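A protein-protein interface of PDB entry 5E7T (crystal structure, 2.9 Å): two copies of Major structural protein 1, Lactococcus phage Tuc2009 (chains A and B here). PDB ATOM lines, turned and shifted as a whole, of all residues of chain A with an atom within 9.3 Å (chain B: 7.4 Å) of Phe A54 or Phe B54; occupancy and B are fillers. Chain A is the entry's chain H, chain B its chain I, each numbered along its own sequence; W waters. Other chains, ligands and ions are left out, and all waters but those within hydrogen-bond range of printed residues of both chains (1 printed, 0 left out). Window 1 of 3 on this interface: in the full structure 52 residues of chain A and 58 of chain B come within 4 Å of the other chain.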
ATOM      1  N   PHE A  44       5.302  -3.297 -11.811  1.00  0.00           N
ATOM      2  CA  PHE A  44       5.640  -4.707 -11.598  1.00  0.00           C
ATOM      3  C   PHE A  44       5.044  -5.602 -12.696  1.00  0.00           C
ATOM      4  O   PHE A  44       3.824  -5.675 -12.832  1.00  0.00           O
ATOM      5  CB  PHE A  44       5.182  -5.171 -10.204  1.00  0.00           C
ATOM      6  CG  PHE A  44       5.910  -4.570  -9.021  1.00  0.00           C
ATOM      7  CD1 PHE A  44       5.469  -3.386  -8.438  1.00  0.00           C
ATOM      8  CD2 PHE A  44       7.008  -5.213  -8.457  1.00  0.00           C
ATOM      9  CE1 PHE A  44       6.148  -2.832  -7.342  1.00  0.00           C
ATOM     10  CE2 PHE A  44       7.670  -4.670  -7.348  1.00  0.00           C
ATOM     11  CZ  PHE A  44       7.243  -3.480  -6.806  1.00  0.00           C
ATOM     12  N   SER A  45       5.909  -6.275 -13.477  1.00  0.00           N
ATOM     13  CA  SER A  45       5.538  -7.194 -14.564  1.00  0.00           C
ATOM     14  C   SER A  45       4.812  -8.437 -14.041  1.00  0.00           C
ATOM     15  O   SER A  45       3.777  -8.808 -14.601  1.00  0.00           O
ATOM     16  CB  SER A  45       6.773  -7.647 -15.340  1.00  0.00           C
ATOM     17  OG  SER A  45       7.468  -6.567 -15.937  1.00  0.00           O
ATOM     18  N   GLY A  46       5.371  -9.067 -12.998  1.00  0.00           N
ATOM     19  CA  GLY A  46       4.842 -10.296 -12.414  1.00  0.00           C
ATOM     20  C   GLY A  46       3.834 -10.109 -11.304  1.00  0.00           C
ATOM     21  O   GLY A  46       3.268  -9.021 -11.142  1.00  0.00           O
ATOM     22  N   ASP A  47       3.601 -11.192 -10.536  1.00  0.00           N
ATOM     23  CA  ASP A  47       2.672 -11.211  -9.401  1.00  0.00           C
ATOM     24  C   ASP A  47       3.293 -10.521  -8.193  1.00  0.00           C
ATOM     25  O   ASP A  47       4.499 -10.610  -7.987  1.00  0.00           O
ATOM     26  CB  ASP A  47       2.300 -12.660  -9.021  1.00  0.00           C
ATOM     27  CG  ASP A  47       1.581 -13.489 -10.079  1.00  0.00           C
ATOM     28  OD1 ASP A  47       1.253 -12.934 -11.153  1.00  0.00           O
ATOM     29  OD2 ASP A  47       1.341 -14.691  -9.827  1.00  0.00           O
ATOM     30  N   VAL A  48       2.458  -9.846  -7.391  1.00  0.00           N
ATOM     31  CA  VAL A  48       2.848  -9.138  -6.164  1.00  0.00           C
ATOM     32  C   VAL A  48       1.900  -9.552  -5.024  1.00  0.00           C
ATOM     33  O   VAL A  48       0.676  -9.503  -5.177  1.00  0.00           O
ATOM     34  CB  VAL A  48       2.909  -7.592  -6.348  1.00  0.00           C
ATOM     35  CG1 VAL A  48       3.091  -6.869  -5.022  1.00  0.00           C
ATOM     36  CG2 VAL A  48       4.011  -7.191  -7.319  1.00  0.00           C
ATOM     37  N   SER A  49       2.481  -9.966  -3.887  1.00  0.00           N
ATOM     38  CA  SER A  49       1.741 -10.381  -2.695  1.00  0.00           C
ATOM     39  C   SER A  49       2.231  -9.573  -1.495  1.00  0.00           C
ATOM     40  O   SER A  49       3.442  -9.407  -1.325  1.00  0.00           O
ATOM     41  CB  SER A  49       1.945 -11.874  -2.440  1.00  0.00           C
ATOM     42  OG  SER A  49       1.449 -12.677  -3.501  1.00  0.00           O
ATOM     43  N   VAL A  50       1.300  -9.058  -0.677  1.00  0.00           N
ATOM     44  CA  VAL A  50       1.615  -8.293   0.539  1.00  0.00           C
ATOM     45  C   VAL A  50       1.055  -9.035   1.775  1.00  0.00           C
ATOM     46  O   VAL A  50      -0.152  -8.981   2.045  1.00  0.00           O
ATOM     47  CB  VAL A  50       1.166  -6.801   0.474  1.00  0.00           C
ATOM     48  CG1 VAL A  50       1.551  -6.042   1.744  1.00  0.00           C
ATOM     49  CG2 VAL A  50       1.738  -6.104  -0.753  1.00  0.00           C
ATOM     50  N   ASP A  51       1.943  -9.735   2.503  1.00  0.00           N
ATOM     51  CA  ASP A  51       1.618 -10.481   3.714  1.00  0.00           C
ATOM     52  C   ASP A  51       1.292  -9.548   4.886  1.00  0.00           C
ATOM     53  O   ASP A  51       0.445  -9.878   5.722  1.00  0.00           O
ATOM     54  CB  ASP A  51       2.764 -11.439   4.078  1.00  0.00           C
ATOM     55  CG  ASP A  51       3.005 -12.574   3.091  1.00  0.00           C
ATOM     56  OD1 ASP A  51       2.104 -12.846   2.253  1.00  0.00           O
ATOM     57  OD2 ASP A  51       4.066 -13.229   3.193  1.00  0.00           O
ATOM     58  N   GLY A  52       1.947  -8.390   4.918  1.00  0.00           N
ATOM     59  CA  GLY A  52       1.751  -7.382   5.953  1.00  0.00           C
ATOM     60  C   GLY A  52       0.581  -6.471   5.671  1.00  0.00           C
ATOM     61  O   GLY A  52      -0.333  -6.833   4.921  1.00  0.00           O
ATOM     62  N   ASP A  53       0.615  -5.277   6.263  1.00  0.00           N
ATOM     63  CA  ASP A  53      -0.454  -4.304   6.109  1.00  0.00           C
ATOM     64  C   ASP A  53      -0.324  -3.467   4.843  1.00  0.00           C
ATOM     65  O   ASP A  53       0.504  -2.549   4.788  1.00  0.00           O
ATOM     66  CB  ASP A  53      -0.587  -3.425   7.364  1.00  0.00           C
ATOM     67  CG  ASP A  53      -1.353  -4.077   8.501  1.00  0.00           C
ATOM     68  OD1 ASP A  53      -2.580  -4.271   8.355  1.00  0.00           O
ATOM     69  OD2 ASP A  53      -0.735  -4.348   9.557  1.00  0.00           O
ATOM     70  N   PHE A  54      -1.154  -3.790   3.821  1.00  0.00           N
ATOM     71  CA  PHE A  54      -1.197  -3.047   2.559  1.00  0.00           C
ATOM     72  C   PHE A  54      -2.022  -1.769   2.682  1.00  0.00           C
ATOM     73  O   PHE A  54      -3.198  -1.792   3.071  1.00  0.00           O
ATOM     74  CB  PHE A  54      -1.680  -3.893   1.367  1.00  0.00           C
ATOM     75  CG  PHE A  54      -1.545  -3.170   0.038  1.00  0.00           C
ATOM     76  CD1 PHE A  54      -0.295  -2.986  -0.555  1.00  0.00           C
ATOM     77  CD2 PHE A  54      -2.666  -2.676  -0.623  1.00  0.00           C
ATOM     78  CE1 PHE A  54      -0.173  -2.308  -1.774  1.00  0.00           C
ATOM     79  CE2 PHE A  54      -2.541  -2.013  -1.852  1.00  0.00           C
ATOM     80  CZ  PHE A  54      -1.295  -1.825  -2.411  1.00  0.00           C
ATOM     81  N   THR A  55      -1.387  -0.659   2.338  1.00  0.00           N
ATOM     82  CA  THR A  55      -1.979   0.662   2.384  1.00  0.00           C
ATOM     83  C   THR A  55      -1.961   1.198   0.962  1.00  0.00           C
ATOM     84  O   THR A  55      -0.942   1.116   0.272  1.00  0.00           O
ATOM     85  CB  THR A  55      -1.191   1.549   3.368  1.00  0.00           C
ATOM     86  OG1 THR A  55      -0.987   0.850   4.601  1.00  0.00           O
ATOM     87  CG2 THR A  55      -1.850   2.892   3.624  1.00  0.00           C
ATOM     88  N   MET A  56      -3.112   1.696   0.514  1.00  0.00           N
ATOM     89  CA  MET A  56      -3.287   2.334  -0.793  1.00  0.00           C
ATOM     90  C   MET A  56      -4.130   3.609  -0.580  1.00  0.00           C
ATOM     91  O   MET A  56      -5.008   3.629   0.295  1.00  0.00           O
ATOM     92  CB  MET A  56      -3.894   1.373  -1.856  1.00  0.00           C
ATOM     93  CG  MET A  56      -5.349   0.972  -1.612  1.00  0.00           C
ATOM     94  SD  MET A  56      -6.123  -0.072  -2.874  1.00  0.00           S
ATOM     95  CE  MET A  56      -6.268  -1.622  -1.980  1.00  0.00           C
ATOM     96  N   LYS A  57      -3.807   4.689  -1.303  1.00  0.00           N
ATOM     97  CA  LYS A  57      -4.588   5.916  -1.189  1.00  0.00           C
ATOM     98  C   LYS A  57      -5.802   5.789  -2.135  1.00  0.00           C
ATOM     99  O   LYS A  57      -5.744   5.007  -3.099  1.00  0.00           O
ATOM    100  CB  LYS A  57      -3.740   7.159  -1.508  1.00  0.00           C
ATOM    101  CG  LYS A  57      -3.060   7.759  -0.291  1.00  0.00           C
ATOM    102  CD  LYS A  57      -2.429   9.112  -0.617  1.00  0.00           C
ATOM    103  CE  LYS A  57      -1.853   9.826   0.589  1.00  0.00           C
ATOM    104  NZ  LYS A  57      -0.616   9.184   1.114  1.00  0.00           N
ATOM    105  N   PHE A  59      -8.995   4.254  -2.368  1.00  0.00           N
ATOM    106  CA  PHE A  59      -9.474   2.975  -2.925  1.00  0.00           C
ATOM    107  C   PHE A  59     -10.843   3.088  -3.634  1.00  0.00           C
ATOM    108  O   PHE A  59     -10.973   2.527  -4.722  1.00  0.00           O
ATOM    109  CB  PHE A  59      -9.466   1.817  -1.890  1.00  0.00           C
ATOM    110  CG  PHE A  59     -10.337   0.610  -2.214  1.00  0.00           C
ATOM    111  CD1 PHE A  59     -10.050  -0.211  -3.306  1.00  0.00           C
ATOM    112  CD2 PHE A  59     -11.425   0.282  -1.412  1.00  0.00           C
ATOM    113  CE1 PHE A  59     -10.872  -1.302  -3.622  1.00  0.00           C
ATOM    114  CE2 PHE A  59     -12.230  -0.825  -1.712  1.00  0.00           C
ATOM    115  CZ  PHE A  59     -11.956  -1.600  -2.821  1.00  0.00           C
ATOM    116  N   TYR A  63     -11.243   2.211  -7.483  1.00  0.00           N
ATOM    117  CA  TYR A  63     -11.891   0.933  -7.832  1.00  0.00           C
ATOM    118  C   TYR A  63     -13.443   0.875  -7.868  1.00  0.00           C
ATOM    119  O   TYR A  63     -13.947  -0.096  -8.434  1.00  0.00           O
ATOM    120  CB  TYR A  63     -11.359  -0.200  -6.929  1.00  0.00           C
ATOM    121  CG  TYR A  63      -9.885  -0.440  -7.172  1.00  0.00           C
ATOM    122  CD1 TYR A  63      -9.453  -1.220  -8.242  1.00  0.00           C
ATOM    123  CD2 TYR A  63      -8.916   0.211  -6.409  1.00  0.00           C
ATOM    124  CE1 TYR A  63      -8.095  -1.363  -8.532  1.00  0.00           C
ATOM    125  CE2 TYR A  63      -7.554   0.050  -6.671  1.00  0.00           C
ATOM    126  CZ  TYR A  63      -7.147  -0.738  -7.733  1.00  0.00           C
ATOM    127  OH  TYR A  63      -5.808  -0.871  -8.005  1.00  0.00           O
ATOM    128  N   PHE B  44       6.289   3.623  -0.754  1.00  0.00           N
ATOM    129  CA  PHE B  44       6.463   4.121  -2.120  1.00  0.00           C
ATOM    130  C   PHE B  44       5.924   5.558  -2.263  1.00  0.00           C
ATOM    131  O   PHE B  44       4.733   5.779  -2.093  1.00  0.00           O
ATOM    132  CB  PHE B  44       5.811   3.174  -3.143  1.00  0.00           C
ATOM    133  CG  PHE B  44       6.444   1.810  -3.288  1.00  0.00           C
ATOM    134  CD1 PHE B  44       6.016   0.740  -2.510  1.00  0.00           C
ATOM    135  CD2 PHE B  44       7.441   1.583  -4.235  1.00  0.00           C
ATOM    136  CE1 PHE B  44       6.591  -0.532  -2.659  1.00  0.00           C
ATOM    137  CE2 PHE B  44       8.025   0.312  -4.377  1.00  0.00           C
ATOM    138  CZ  PHE B  44       7.592  -0.738  -3.591  1.00  0.00           C
ATOM    139  N   VAL B  48       2.453   3.173  -8.229  1.00  0.00           N
ATOM    140  CA  VAL B  48       2.781   1.736  -8.253  1.00  0.00           C
ATOM    141  C   VAL B  48       1.728   1.001  -9.087  1.00  0.00           C
ATOM    142  O   VAL B  48       0.527   1.202  -8.873  1.00  0.00           O
ATOM    143  CB  VAL B  48       2.952   1.111  -6.834  1.00  0.00           C
ATOM    144  CG1 VAL B  48       3.073  -0.415  -6.890  1.00  0.00           C
ATOM    145  CG2 VAL B  48       4.152   1.710  -6.113  1.00  0.00           C
ATOM    146  N   SER B  49       2.176   0.160 -10.029  1.00  0.00           N
ATOM    147  CA  SER B  49       1.288  -0.618 -10.882  1.00  0.00           C
ATOM    148  C   SER B  49       1.661  -2.088 -10.818  1.00  0.00           C
ATOM    149  O   SER B  49       2.847  -2.411 -10.879  1.00  0.00           O
ATOM    150  CB  SER B  49       1.356  -0.119 -12.324  1.00  0.00           C
ATOM    151  OG  SER B  49       0.858   1.203 -12.465  1.00  0.00           O
ATOM    152  N   VAL B  50       0.659  -2.979 -10.670  1.00  0.00           N
ATOM    153  CA  VAL B  50       0.877  -4.433 -10.631  1.00  0.00           C
ATOM    154  C   VAL B  50       0.124  -5.103 -11.800  1.00  0.00           C
ATOM    155  O   VAL B  50      -1.095  -5.277 -11.739  1.00  0.00           O
ATOM    156  CB  VAL B  50       0.560  -5.085  -9.249  1.00  0.00           C
ATOM    157  CG1 VAL B  50       0.838  -6.589  -9.264  1.00  0.00           C
ATOM    158  CG2 VAL B  50       1.336  -4.412  -8.121  1.00  0.00           C
ATOM    159  N   ASP B  51       0.859  -5.462 -12.859  1.00  0.00           N
ATOM    160  CA  ASP B  51       0.325  -6.121 -14.053  1.00  0.00           C
ATOM    161  C   ASP B  51      -0.098  -7.574 -13.764  1.00  0.00           C
ATOM    162  O   ASP B  51      -1.054  -8.063 -14.365  1.00  0.00           O
ATOM    163  CB  ASP B  51       1.354  -6.073 -15.208  1.00  0.00           C
ATOM    164  CG  ASP B  51       1.724  -4.684 -15.706  1.00  0.00           C
ATOM    165  OD1 ASP B  51       0.936  -3.735 -15.469  1.00  0.00           O
ATOM    166  OD2 ASP B  51       2.789  -4.550 -16.350  1.00  0.00           O
ATOM    167  N   GLY B  52       0.613  -8.239 -12.856  1.00  0.00           N
ATOM    168  CA  GLY B  52       0.323  -9.612 -12.459  1.00  0.00           C
ATOM    169  C   GLY B  52      -0.744  -9.727 -11.388  1.00  0.00           C
ATOM    170  O   GLY B  52      -1.517  -8.782 -11.151  1.00  0.00           O
ATOM    171  N   ASP B  53      -0.804 -10.912 -10.743  1.00  0.00           N
ATOM    172  CA  ASP B  53      -1.790 -11.206  -9.696  1.00  0.00           C
ATOM    173  C   ASP B  53      -1.436 -10.522  -8.370  1.00  0.00           C
ATOM    174  O   ASP B  53      -0.360 -10.776  -7.817  1.00  0.00           O
ATOM    175  CB  ASP B  53      -1.972 -12.733  -9.506  1.00  0.00           C
ATOM    176  CG  ASP B  53      -2.771 -13.422 -10.599  1.00  0.00           C
ATOM    177  OD1 ASP B  53      -3.937 -13.028 -10.823  1.00  0.00           O
ATOM    178  OD2 ASP B  53      -2.243 -14.383 -11.202  1.00  0.00           O
ATOM    179  N   PHE B  54      -2.336  -9.654  -7.868  1.00  0.00           N
ATOM    180  CA  PHE B  54      -2.122  -8.955  -6.600  1.00  0.00           C
ATOM    181  C   PHE B  54      -2.791  -9.664  -5.390  1.00  0.00           C
ATOM    182  O   PHE B  54      -4.012  -9.590  -5.233  1.00  0.00           O
ATOM    183  CB  PHE B  54      -2.537  -7.467  -6.693  1.00  0.00           C
ATOM    184  CG  PHE B  54      -2.191  -6.680  -5.451  1.00  0.00           C
ATOM    185  CD1 PHE B  54      -0.920  -6.156  -5.275  1.00  0.00           C
ATOM    186  CD2 PHE B  54      -3.117  -6.517  -4.431  1.00  0.00           C
ATOM    187  CE1 PHE B  54      -0.591  -5.465  -4.111  1.00  0.00           C
ATOM    188  CE2 PHE B  54      -2.785  -5.827  -3.269  1.00  0.00           C
ATOM    189  CZ  PHE B  54      -1.526  -5.305  -3.116  1.00  0.00           C
ATOM    190  N   THR B  55      -1.992 -10.323  -4.526  1.00  0.00           N
ATOM    191  CA  THR B  55      -2.514 -10.997  -3.327  1.00  0.00           C
ATOM    192  C   THR B  55      -2.524  -9.991  -2.159  1.00  0.00           C
ATOM    193  O   THR B  55      -1.542  -9.278  -1.957  1.00  0.00           O
ATOM    194  CB  THR B  55      -1.726 -12.302  -3.051  1.00  0.00           C
ATOM    195  OG1 THR B  55      -1.748 -13.138  -4.212  1.00  0.00           O
ATOM    196  CG2 THR B  55      -2.249 -13.079  -1.854  1.00  0.00           C
ATOM    197  N   MET B  56      -3.641  -9.922  -1.416  1.00  0.00           N
ATOM    198  CA  MET B  56      -3.831  -9.013  -0.280  1.00  0.00           C
ATOM    199  C   MET B  56      -4.294  -9.767   0.961  1.00  0.00           C
ATOM    200  O   MET B  56      -5.287 -10.516   0.906  1.00  0.00           O
ATOM    201  CB  MET B  56      -4.900  -7.953  -0.613  1.00  0.00           C
ATOM    202  CG  MET B  56      -4.484  -6.536  -0.346  1.00  0.00           C
ATOM    203  SD  MET B  56      -5.800  -5.327  -0.653  1.00  0.00           S
ATOM    204  CE  MET B  56      -6.309  -5.724  -2.338  1.00  0.00           C
ATOM    205  N   LYS B  57      -3.610  -9.523   2.096  1.00  0.00           N
ATOM    206  CA  LYS B  57      -3.996 -10.112   3.372  1.00  0.00           C
ATOM    207  C   LYS B  57      -5.076  -9.249   3.993  1.00  0.00           C
ATOM    208  O   LYS B  57      -4.913  -8.027   4.093  1.00  0.00           O
ATOM    209  CB  LYS B  57      -2.797 -10.268   4.328  1.00  0.00           C
ATOM    210  CG  LYS B  57      -2.474 -11.722   4.686  1.00  0.00           C
ATOM    211  CD  LYS B  57      -1.644 -12.426   3.590  1.00  0.00           C
ATOM    212  CE  LYS B  57      -1.292 -13.864   3.901  1.00  0.00           C
ATOM    213  NZ  LYS B  57      -2.374 -14.804   3.503  1.00  0.00           N
ATOM    214  N   SER B  62      -9.807  -4.399   6.235  1.00  0.00           N
ATOM    215  CA  SER B  62      -8.952  -3.230   6.003  1.00  0.00           C
ATOM    216  C   SER B  62      -9.496  -2.189   5.012  1.00  0.00           C
ATOM    217  O   SER B  62      -9.037  -1.038   5.056  1.00  0.00           O
ATOM    218  CB  SER B  62      -7.561  -3.680   5.582  1.00  0.00           C
ATOM    219  OG  SER B  62      -7.665  -4.543   4.466  1.00  0.00           O
ATOM    220  N   TYR B  63     -10.467  -2.575   4.137  1.00  0.00           N
ATOM    221  CA  TYR B  63     -11.070  -1.640   3.181  1.00  0.00           C
ATOM    222  C   TYR B  63     -12.613  -1.557   3.274  1.00  0.00           C
ATOM    223  O   TYR B  63     -13.190  -0.589   2.775  1.00  0.00           O
ATOM    224  CB  TYR B  63     -10.588  -1.900   1.746  1.00  0.00           C
ATOM    225  CG  TYR B  63      -9.143  -1.485   1.575  1.00  0.00           C
ATOM    226  CD1 TYR B  63      -8.799  -0.148   1.380  1.00  0.00           C
ATOM    227  CD2 TYR B  63      -8.112  -2.409   1.715  1.00  0.00           C
ATOM    228  CE1 TYR B  63      -7.466   0.256   1.324  1.00  0.00           C
ATOM    229  CE2 TYR B  63      -6.775  -2.019   1.646  1.00  0.00           C
ATOM    230  CZ  TYR B  63      -6.456  -0.685   1.452  1.00  0.00           C
ATOM    231  OH  TYR B  63      -5.137  -0.313   1.384  1.00  0.00           O
ATOM    232  N   ARG B 172     -13.396   2.199   1.855  1.00  0.00           N
ATOM    233  CA  ARG B 172     -12.237   3.065   2.158  1.00  0.00           C
ATOM    234  C   ARG B 172     -11.748   3.903   0.942  1.00  0.00           C
ATOM    235  O   ARG B 172     -11.687   3.368  -0.166  1.00  0.00           O
ATOM    236  CB  ARG B 172     -11.092   2.227   2.749  1.00  0.00           C
ATOM    237  CG  ARG B 172      -9.969   3.059   3.335  1.00  0.00           C
ATOM    238  CD  ARG B 172      -8.961   2.228   4.077  1.00  0.00           C
ATOM    239  NE  ARG B 172      -7.843   3.063   4.518  1.00  0.00           N
ATOM    240  CZ  ARG B 172      -6.749   2.603   5.116  1.00  0.00           C
ATOM    241  NH1 ARG B 172      -6.615   1.304   5.368  1.00  0.00           N
ATOM    242  NH2 ARG B 172      -5.775   3.435   5.460  1.00  0.00           N
HETATM  243  O   HOH W   1       0.491 -13.650  -5.894  1.00  0.00           O
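The guanidinium group of Arg B172 lies within hydrogen-bond range of the backbone carbonyl oxygen of Ser B62 (3.4 Å). The backbone carbonyl oxygen of Tyr B63 lies within hydrogen-bond range of the backbone NH of Arg B172, at 2.9 Å.
Among the printed residues, merely in contact across the chains: Val A48 with Phe B54, Phe A59 with Arg B172, Thr A55 with Tyr B63, Asp A51 with Lys B57, Phe A54 with Phe B54, Ser A45 with Gly B52, Asp A47 with Gly B52, Ser A45 with Asp B51, Val A48 with Val B50, Phe A59 with Tyr B63, Phe A44 with Val B50, Gly A46 with Val B50, Phe A44 with Val B48 and Met A56 with Met B56.
Hydrophobic or aromatic side chains of chain B that line the printed part of chain A: Val B48, Val B50, Phe B54, Met B56 and Tyr B63. Among the printed residues, 25 pairs touch across the chains.
Of chain B, only Phe B54 (3.6 Å) and Tyr B63 (3.0 Å) come within 4 Å of Phe A54. Phe B54 touches two residues of chain A. Thr B55 touches just these residues of chain A: Val A48, Ser A49 and Val A50. Of the printed residues of chain B, Val A50 touches Thr B55 (3.1 Å) and Lys B57 (3.5 Å). Of the printed residues of chain B, Phe A59 touches Tyr B63 and Arg B172. Of the printed residues of chain A, Asp B53 touches Asp A47 (2.9 Å) and Val A48 (3.0 Å). Of the printed residues of chain B, Asp A47 touches Gly B52 and Asp B53. Tyr A63 touches none of the printed residues of chain B. Gly A52 touches none of the printed residues of chain B. The nearest residue of chain B that does not touch Phe A54 is Met B56 (4.1 Å). The nearest printed residue of chain A that does not touch Gly B52 is Phe A44 (4.1 Å).
Val A48 touches Val B50, but with the chains exchanged Val A50 does not touch Val B48 (8.5 Å). Ser A49 touches Thr B55, but with the chains exchanged Thr A55 does not touch Ser B49 (10.8 Å). Val A50 touches Lys B57, but with the chains exchanged Lys A57 does not touch Val B50 (12.5 Å). Asp A51 touches Lys B57, but with the chains exchanged Lys A57 does not touch Asp B51 (15.8 Å).
Water W1 lies within hydrogen-bond range of the side-chain hydroxyl of Ser A49 (2.8 Å) and the side-chain hydroxyl of Thr B55 (2.8 Å).
The backbone NH (N) of Phe A44 is in hydrogen-bond range of the backbone carbonyl oxygen (O) of Ser B49, at 2.8 Å. The backbone carbonyl oxygen (O) of Phe A44 is in hydrogen-bond range of the backbone NH (N) of Asp B51 (3.0 Å). O of Gly A46 is in hydrogen-bond range of N of Gly B52. N of Asp B53 sits at hydrogen-bond distance from OD1 of Asp A47, at 2.9 Å. The backbone carbonyl oxygen (O) of Asp B53 lies within hydrogen-bond range of the backbone NH (N) of Val A48 (3.0 Å). The backbone NH (N) of Thr B55 lies within hydrogen-bond range of the backbone carbonyl oxygen (O) of Val A48. The side-chain hydroxyl (OG) of Ser A49 sits close to the side-chain hydroxyl (OG1) of Thr B55 (3.3 Å). The backbone carbonyl oxygen (O) of Thr B55 sits at hydrogen-bond distance from the backbone NH (N) of Val A50 (3.1 Å). N of Lys B57 lies close to O of Val A50, at 3.5 Å. The backbone carbonyl oxygen (O) of Phe A54 sits at hydrogen-bond distance from the side-chain hydroxyl (OH) of Tyr B63 (3.0 Å). N of Met A56 lies within hydrogen-bond range of OH of Tyr B63 (3.0 Å).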
